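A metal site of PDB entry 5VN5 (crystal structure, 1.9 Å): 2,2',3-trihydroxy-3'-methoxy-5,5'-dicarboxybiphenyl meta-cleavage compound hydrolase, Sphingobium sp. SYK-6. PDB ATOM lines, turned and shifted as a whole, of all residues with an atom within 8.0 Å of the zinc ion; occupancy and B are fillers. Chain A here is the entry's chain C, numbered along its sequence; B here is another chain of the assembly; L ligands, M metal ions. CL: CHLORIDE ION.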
ATOM      1  N   HIS A   6      -5.501  17.475  -5.144  1.00  0.00           N
ATOM      2  CA  HIS A   6      -5.351  17.104  -6.561  1.00  0.00           C
ATOM      3  C   HIS A   6      -6.556  16.268  -6.996  1.00  0.00           C
ATOM      4  O   HIS A   6      -6.515  15.040  -7.030  1.00  0.00           O
ATOM      5  CB  HIS A   6      -4.043  16.353  -6.778  1.00  0.00           C
ATOM      6  CG  HIS A   6      -3.661  16.201  -8.214  1.00  0.00           C
ATOM      7  ND1 HIS A   6      -2.363  16.379  -8.647  1.00  0.00           N
ATOM      8  CD2 HIS A   6      -4.386  15.893  -9.315  1.00  0.00           C
ATOM      9  CE1 HIS A   6      -2.311  16.183  -9.957  1.00  0.00           C
ATOM     10  NE2 HIS A   6      -3.522  15.901 -10.386  1.00  0.00           N
ATOM     11  N   GLY A   7      -7.642  16.941  -7.349  1.00  0.00           N
ATOM     12  CA  GLY A   7      -8.775  16.291  -7.963  1.00  0.00           C
ATOM     13  C   GLY A   7      -9.185  17.056  -9.211  1.00  0.00           C
ATOM     14  O   GLY A   7      -8.908  18.238  -9.361  1.00  0.00           O
ATOM     15  N   HIS A   8      -9.828  16.341 -10.123  1.00  0.00           N
ATOM     16  CA  HIS A   8     -10.315  16.958 -11.348  1.00  0.00           C
ATOM     17  C   HIS A   8     -11.833  16.827 -11.429  1.00  0.00           C
ATOM     18  O   HIS A   8     -12.406  15.850 -10.964  1.00  0.00           O
ATOM     19  CB  HIS A   8      -9.645  16.346 -12.573  1.00  0.00           C
ATOM     20  CG  HIS A   8      -8.146  16.438 -12.518  1.00  0.00           C
ATOM     21  ND1 HIS A   8      -7.497  17.613 -12.252  1.00  0.00           N
ATOM     22  CD2 HIS A   8      -7.187  15.498 -12.657  1.00  0.00           C
ATOM     23  CE1 HIS A   8      -6.191  17.407 -12.259  1.00  0.00           C
ATOM     24  NE2 HIS A   8      -5.981  16.129 -12.506  1.00  0.00           N
ATOM     25  N   SER A  70      -9.912  20.890 -10.160  1.00  0.00           N
ATOM     26  CA  SER A  70      -9.421  21.653 -11.275  1.00  0.00           C
ATOM     27  C   SER A  70      -9.919  21.007 -12.565  1.00  0.00           C
ATOM     28  O   SER A  70     -10.543  19.937 -12.528  1.00  0.00           O
ATOM     29  CB  SER A  70      -7.889  21.682 -11.217  1.00  0.00           C
ATOM     30  OG  SER A  70      -7.389  20.366 -11.206  1.00  0.00           O
ATOM     31  N   PRO A  71      -9.689  21.613 -13.730  1.00  0.00           N
ATOM     32  CA  PRO A  71     -10.109  20.980 -14.990  1.00  0.00           C
ATOM     33  C   PRO A  71      -9.468  19.598 -15.153  1.00  0.00           C
ATOM     34  O   PRO A  71      -8.407  19.307 -14.591  1.00  0.00           O
ATOM     35  CB  PRO A  71      -9.603  21.950 -16.062  1.00  0.00           C
ATOM     36  CG  PRO A  71      -9.554  23.283 -15.371  1.00  0.00           C
ATOM     37  CD  PRO A  71      -9.150  22.967 -13.933  1.00  0.00           C
ATOM     38  N   ARG A  72     -10.114  18.765 -15.961  1.00  0.00           N
ATOM     39  CA  ARG A  72      -9.482  17.511 -16.418  1.00  0.00           C
ATOM     40  C   ARG A  72      -8.408  17.899 -17.425  1.00  0.00           C
ATOM     41  O   ARG A  72      -8.739  18.296 -18.553  1.00  0.00           O
ATOM     42  CB  ARG A  72     -10.500  16.581 -17.065  1.00  0.00           C
ATOM     43  CG  ARG A  72     -11.525  15.972 -16.080  1.00  0.00           C
ATOM     44  CD  ARG A  72     -10.944  14.759 -15.368  1.00  0.00           C
ATOM     45  NE  ARG A  72     -11.805  14.272 -14.283  1.00  0.00           N
ATOM     46  CZ  ARG A  72     -11.518  13.212 -13.518  1.00  0.00           C
ATOM     47  NH1 ARG A  72     -10.399  12.524 -13.710  1.00  0.00           N
ATOM     48  NH2 ARG A  72     -12.357  12.841 -12.551  1.00  0.00           N
ATOM     49  N   PRO A  73      -7.121  17.819 -17.071  1.00  0.00           N
ATOM     50  CA  PRO A  73      -6.108  18.449 -17.915  1.00  0.00           C
ATOM     51  C   PRO A  73      -6.032  17.889 -19.328  1.00  0.00           C
ATOM     52  O   PRO A  73      -5.794  18.655 -20.284  1.00  0.00           O
ATOM     53  CB  PRO A  73      -4.813  18.199 -17.121  1.00  0.00           C
ATOM     54  CG  PRO A  73      -5.262  18.209 -15.716  1.00  0.00           C
ATOM     55  CD  PRO A  73      -6.529  17.395 -15.775  1.00  0.00           C
ATOM     56  N   PHE A  74      -6.229  16.580 -19.513  1.00  0.00           N
ATOM     57  CA  PHE A  74      -6.048  16.012 -20.843  1.00  0.00           C
ATOM     58  C   PHE A  74      -7.138  16.426 -21.818  1.00  0.00           C
ATOM     59  O   PHE A  74      -7.011  16.142 -23.010  1.00  0.00           O
ATOM     60  CB  PHE A  74      -5.961  14.478 -20.760  1.00  0.00           C
ATOM     61  CG  PHE A  74      -7.285  13.788 -20.651  1.00  0.00           C
ATOM     62  CD1 PHE A  74      -8.244  14.191 -19.735  1.00  0.00           C
ATOM     63  CD2 PHE A  74      -7.587  12.726 -21.462  1.00  0.00           C
ATOM     64  CE1 PHE A  74      -9.460  13.537 -19.633  1.00  0.00           C
ATOM     65  CE2 PHE A  74      -8.817  12.070 -21.370  1.00  0.00           C
ATOM     66  CZ  PHE A  74      -9.741  12.481 -20.454  1.00  0.00           C
ATOM     67  N   LEU A 141      -3.794  25.673 -12.489  1.00  0.00           N
ATOM     68  CA  LEU A 141      -2.975  24.666 -13.144  1.00  0.00           C
ATOM     69  C   LEU A 141      -2.074  25.352 -14.160  1.00  0.00           C
ATOM     70  O   LEU A 141      -2.522  26.180 -14.951  1.00  0.00           O
ATOM     71  CB  LEU A 141      -3.823  23.619 -13.859  1.00  0.00           C
ATOM     72  CG  LEU A 141      -4.777  22.782 -13.022  1.00  0.00           C
ATOM     73  CD1 LEU A 141      -5.250  21.598 -13.834  1.00  0.00           C
ATOM     74  CD2 LEU A 141      -4.128  22.335 -11.730  1.00  0.00           C
ATOM     75  N   HIS A 177      -0.035  25.072  -9.867  1.00  0.00           N
ATOM     76  CA  HIS A 177       0.002  23.620  -9.701  1.00  0.00           C
ATOM     77  C   HIS A 177       0.428  23.042 -11.038  1.00  0.00           C
ATOM     78  O   HIS A 177      -0.381  23.007 -11.972  1.00  0.00           O
ATOM     79  CB  HIS A 177      -1.377  23.133  -9.303  1.00  0.00           C
ATOM     80  CG  HIS A 177      -1.412  21.786  -8.659  1.00  0.00           C
ATOM     81  ND1 HIS A 177      -2.517  21.344  -7.966  1.00  0.00           N
ATOM     82  CD2 HIS A 177      -0.503  20.785  -8.612  1.00  0.00           C
ATOM     83  CE1 HIS A 177      -2.270  20.125  -7.494  1.00  0.00           C
ATOM     84  NE2 HIS A 177      -1.055  19.765  -7.873  1.00  0.00           N
ATOM     85  N   ILE A 178       1.702  22.622 -11.144  1.00  0.00           N
ATOM     86  CA  ILE A 178       2.243  22.139 -12.409  1.00  0.00           C
ATOM     87  C   ILE A 178       1.473  20.923 -12.887  1.00  0.00           C
ATOM     88  O   ILE A 178       1.400  19.906 -12.187  1.00  0.00           O
ATOM     89  CB  ILE A 178       3.732  21.787 -12.268  1.00  0.00           C
ATOM     90  CG1 ILE A 178       4.550  22.968 -11.723  1.00  0.00           C
ATOM     91  CG2 ILE A 178       4.301  21.290 -13.619  1.00  0.00           C
ATOM     92  CD1 ILE A 178       4.546  24.181 -12.605  1.00  0.00           C
ATOM     93  N   HIS A 179       0.964  20.996 -14.112  1.00  0.00           N
ATOM     94  CA  HIS A 179       0.224  19.872 -14.685  1.00  0.00           C
ATOM     95  C   HIS A 179       0.228  20.001 -16.191  1.00  0.00           C
ATOM     96  O   HIS A 179      -0.251  21.001 -16.731  1.00  0.00           O
ATOM     97  CB  HIS A 179      -1.213  19.856 -14.158  1.00  0.00           C
ATOM     98  CG  HIS A 179      -1.803  18.499 -14.071  1.00  0.00           C
ATOM     99  ND1 HIS A 179      -1.843  17.627 -15.135  1.00  0.00           N
ATOM    100  CD2 HIS A 179      -2.372  17.842 -13.023  1.00  0.00           C
ATOM    101  CE1 HIS A 179      -2.432  16.503 -14.752  1.00  0.00           C
ATOM    102  NE2 HIS A 179      -2.732  16.601 -13.479  1.00  0.00           N
ATOM    103  N   ALA A 180       0.765  18.996 -16.892  1.00  0.00           N
ATOM    104  CA  ALA A 180       0.673  18.963 -18.348  1.00  0.00           C
ATOM    105  C   ALA A 180      -0.752  18.583 -18.762  1.00  0.00           C
ATOM    106  O   ALA A 180      -1.584  18.186 -17.948  1.00  0.00           O
ATOM    107  CB  ALA A 180       1.696  17.988 -18.924  1.00  0.00           C
ATOM    108  N   PHE A 194       2.391  13.304 -18.560  1.00  0.00           N
ATOM    109  CA  PHE A 194       2.287  14.007 -17.280  1.00  0.00           C
ATOM    110  C   PHE A 194       3.594  13.931 -16.501  1.00  0.00           C
ATOM    111  O   PHE A 194       4.088  14.936 -15.974  1.00  0.00           O
ATOM    112  CB  PHE A 194       1.193  13.397 -16.397  1.00  0.00           C
ATOM    113  CG  PHE A 194      -0.233  13.724 -16.817  1.00  0.00           C
ATOM    114  CD1 PHE A 194      -0.508  14.726 -17.717  1.00  0.00           C
ATOM    115  CD2 PHE A 194      -1.303  13.010 -16.265  1.00  0.00           C
ATOM    116  CE1 PHE A 194      -1.846  15.018 -18.085  1.00  0.00           C
ATOM    117  CE2 PHE A 194      -2.637  13.310 -16.630  1.00  0.00           C
ATOM    118  CZ  PHE A 194      -2.894  14.306 -17.534  1.00  0.00           C
ATOM    119  N   GLU A 198       6.344  16.893 -15.677  1.00  0.00           N
ATOM    120  CA  GLU A 198       6.634  17.287 -14.308  1.00  0.00           C
ATOM    121  C   GLU A 198       8.130  17.261 -14.062  1.00  0.00           C
ATOM    122  O   GLU A 198       8.660  18.113 -13.353  1.00  0.00           O
ATOM    123  CB  GLU A 198       5.942  16.369 -13.314  1.00  0.00           C
ATOM    124  CG  GLU A 198       4.459  16.614 -13.240  1.00  0.00           C
ATOM    125  CD  GLU A 198       3.653  15.374 -13.003  1.00  0.00           C
ATOM    126  OE1 GLU A 198       4.253  14.305 -12.756  1.00  0.00           O
ATOM    127  OE2 GLU A 198       2.421  15.489 -13.054  1.00  0.00           O
ATOM    128  N   SER A 222       2.796  18.253  -9.477  1.00  0.00           N
ATOM    129  CA  SER A 222       1.922  17.102  -9.458  1.00  0.00           C
ATOM    130  C   SER A 222       2.699  15.783  -9.423  1.00  0.00           C
ATOM    131  O   SER A 222       3.851  15.687  -9.847  1.00  0.00           O
ATOM    132  CB  SER A 222       1.018  17.110 -10.702  1.00  0.00           C
ATOM    133  OG  SER A 222       0.006  18.105 -10.587  1.00  0.00           O
ATOM    134  N   HIS A 223       2.027  14.755  -8.893  1.00  0.00           N
ATOM    135  CA  HIS A 223       2.499  13.372  -8.950  1.00  0.00           C
ATOM    136  C   HIS A 223       3.893  13.229  -8.340  1.00  0.00           C
ATOM    137  O   HIS A 223       4.797  12.607  -8.917  1.00  0.00           O
ATOM    138  CB  HIS A 223       2.484  12.851 -10.392  1.00  0.00           C
ATOM    139  CG  HIS A 223       1.128  12.945 -11.038  1.00  0.00           C
ATOM    140  ND1 HIS A 223       0.849  13.846 -12.035  1.00  0.00           N
ATOM    141  CD2 HIS A 223      -0.023  12.263 -10.813  1.00  0.00           C
ATOM    142  CE1 HIS A 223      -0.412  13.724 -12.401  1.00  0.00           C
ATOM    143  NE2 HIS A 223      -0.968  12.768 -11.678  1.00  0.00           N
ATOM    144  N   ASP A 256       2.728  17.393  -4.531  1.00  0.00           N
ATOM    145  CA  ASP A 256       1.578  16.628  -4.057  1.00  0.00           C
ATOM    146  C   ASP A 256       1.936  15.135  -4.030  1.00  0.00           C
ATOM    147  O   ASP A 256       2.941  14.704  -4.591  1.00  0.00           O
ATOM    148  CB  ASP A 256       0.314  16.934  -4.885  1.00  0.00           C
ATOM    149  CG  ASP A 256       0.290  16.318  -6.279  1.00  0.00           C
ATOM    150  OD1 ASP A 256       0.808  15.202  -6.512  1.00  0.00           O
ATOM    151  OD2 ASP A 256      -0.366  16.942  -7.146  1.00  0.00           O
ATOM    152  N   VAL A 258       0.365  12.418  -5.201  1.00  0.00           N
ATOM    153  CA  VAL A 258      -0.357  11.522  -6.094  1.00  0.00           C
ATOM    154  C   VAL A 258       0.637  10.491  -6.581  1.00  0.00           C
ATOM    155  O   VAL A 258       1.215  10.631  -7.674  1.00  0.00           O
ATOM    156  CB  VAL A 258      -1.054  12.240  -7.255  1.00  0.00           C
ATOM    157  CG1 VAL A 258      -1.848  11.230  -8.068  1.00  0.00           C
ATOM    158  CG2 VAL A 258      -1.975  13.328  -6.729  1.00  0.00           C
ATOM    159  N   TYR A 260       0.894   6.024  -6.134  1.00  0.00           N
ATOM    160  CA  TYR A 260       0.025   4.906  -5.752  1.00  0.00           C
ATOM    161  C   TYR A 260       0.795   3.686  -5.270  1.00  0.00           C
ATOM    162  O   TYR A 260       0.228   2.590  -5.228  1.00  0.00           O
ATOM    163  CB  TYR A 260      -0.877   4.521  -6.934  1.00  0.00           C
ATOM    164  CG  TYR A 260      -1.723   5.670  -7.448  1.00  0.00           C
ATOM    165  CD1 TYR A 260      -1.714   6.015  -8.798  1.00  0.00           C
ATOM    166  CD2 TYR A 260      -2.512   6.428  -6.596  1.00  0.00           C
ATOM    167  CE1 TYR A 260      -2.475   7.068  -9.276  1.00  0.00           C
ATOM    168  CE2 TYR A 260      -3.281   7.479  -7.062  1.00  0.00           C
ATOM    169  CZ  TYR A 260      -3.269   7.796  -8.403  1.00  0.00           C
ATOM    170  OH  TYR A 260      -4.038   8.852  -8.878  1.00  0.00           O
ATOM    171  N   SER A 281      -4.665  12.850  -4.334  1.00  0.00           N
ATOM    172  CA  SER A 281      -4.934  11.484  -4.776  1.00  0.00           C
ATOM    173  C   SER A 281      -5.405  11.344  -6.215  1.00  0.00           C
ATOM    174  O   SER A 281      -5.308  10.238  -6.759  1.00  0.00           O
ATOM    175  CB  SER A 281      -6.000  10.844  -3.876  1.00  0.00           C
ATOM    176  OG  SER A 281      -7.280  11.356  -4.222  1.00  0.00           O
ATOM    177  N   GLU A 282      -5.932  12.399  -6.847  1.00  0.00           N
ATOM    178  CA  GLU A 282      -6.525  12.313  -8.196  1.00  0.00           C
ATOM    179  C   GLU A 282      -7.719  11.380  -8.236  1.00  0.00           C
ATOM    180  O   GLU A 282      -8.029  10.831  -9.298  1.00  0.00           O
ATOM    181  CB  GLU A 282      -5.521  11.863  -9.256  1.00  0.00           C
ATOM    182  CG  GLU A 282      -5.741  12.503 -10.664  1.00  0.00           C
ATOM    183  CD  GLU A 282      -6.279  11.555 -11.751  1.00  0.00           C
ATOM    184  OE1 GLU A 282      -7.314  11.902 -12.368  1.00  0.00           O
ATOM    185  OE2 GLU A 282      -5.697  10.490 -12.013  1.00  0.00           O
ATOM    186  N   VAL A 286      -7.025   7.967 -12.604  1.00  0.00           N
ATOM    187  CA  VAL A 286      -6.100   6.929 -13.054  1.00  0.00           C
ATOM    188  C   VAL A 286      -5.968   5.840 -12.002  1.00  0.00           C
ATOM    189  O   VAL A 286      -5.899   4.652 -12.328  1.00  0.00           O
ATOM    190  CB  VAL A 286      -4.739   7.559 -13.411  1.00  0.00           C
ATOM    191  CG1 VAL A 286      -3.757   6.519 -13.891  1.00  0.00           C
ATOM    192  CG2 VAL A 286      -4.909   8.656 -14.500  1.00  0.00           C
ATOM    193  N   ARG B 234       0.774   4.208 -10.896  1.00  0.00           N
ATOM    194  CA  ARG B 234      -0.210   4.745 -11.830  1.00  0.00           C
ATOM    195  C   ARG B 234      -0.268   3.918 -13.114  1.00  0.00           C
ATOM    196  O   ARG B 234      -1.341   3.796 -13.728  1.00  0.00           O
ATOM    197  CB  ARG B 234       0.097   6.213 -12.157  1.00  0.00           C
ATOM    198  CG  ARG B 234       1.398   6.411 -12.953  1.00  0.00           C
ATOM    199  CD  ARG B 234       1.717   7.906 -13.182  1.00  0.00           C
ATOM    200  NE  ARG B 234       0.619   8.594 -13.866  1.00  0.00           N
ATOM    201  CZ  ARG B 234      -0.416   9.161 -13.265  1.00  0.00           C
ATOM    202  NH1 ARG B 234      -0.540   9.160 -11.932  1.00  0.00           N
ATOM    203  NH2 ARG B 234      -1.347   9.736 -13.993  1.00  0.00           N
HETATM  204 CL    CL L   1      -3.891  13.728 -13.003  1.00  0.00          CL
HETATM  205 ZN    ZN M   1      -4.080  15.465 -12.378  1.00  0.00          ZN
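Glu 282 touches the zinc ion (CG to ZN, 3.8 Å). The nearest printed residue that does not touch the zinc ion is His 223 (4.1 Å).
The zinc ion is bound by a chlorine (CL) of the ligand (1.9 Å), a ring nitrogen (NE2) of His 8 (2.0 Å), a ring nitrogen (NE2) of His 179 (2.1 Å) and a ring nitrogen (NE2) of His 6 (2.1 Å).
A ring nitrogen (ND1) of His 8 sits at hydrogen-bond distance from the side-chain hydroxyl of Ser 70 (2.9 Å). ND1 of His 8 is in hydrogen-bond range of O of Pro 71, at 3.0 Å. The backbone carbonyl oxygen (O) of His 8 lies within hydrogen-bond range of the guanidinium group (NH2) of Arg 72 (3.4 Å). The backbone NH (N) of Glu 282 is in hydrogen-bond range of the backbone carbonyl oxygen (O) of His 6 (2.7 Å). ND1 of His 6 sits at hydrogen-bond distance from OD2 of Asp 256 (2.6 Å). OE1 of Glu 282 is in salt-bridge range of NH1 of Arg 72, 3.4 Å away. The side-chain carboxylate (OE2) of Glu 282 is in hydrogen-bond range of the backbone NH (N) of Val 286.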
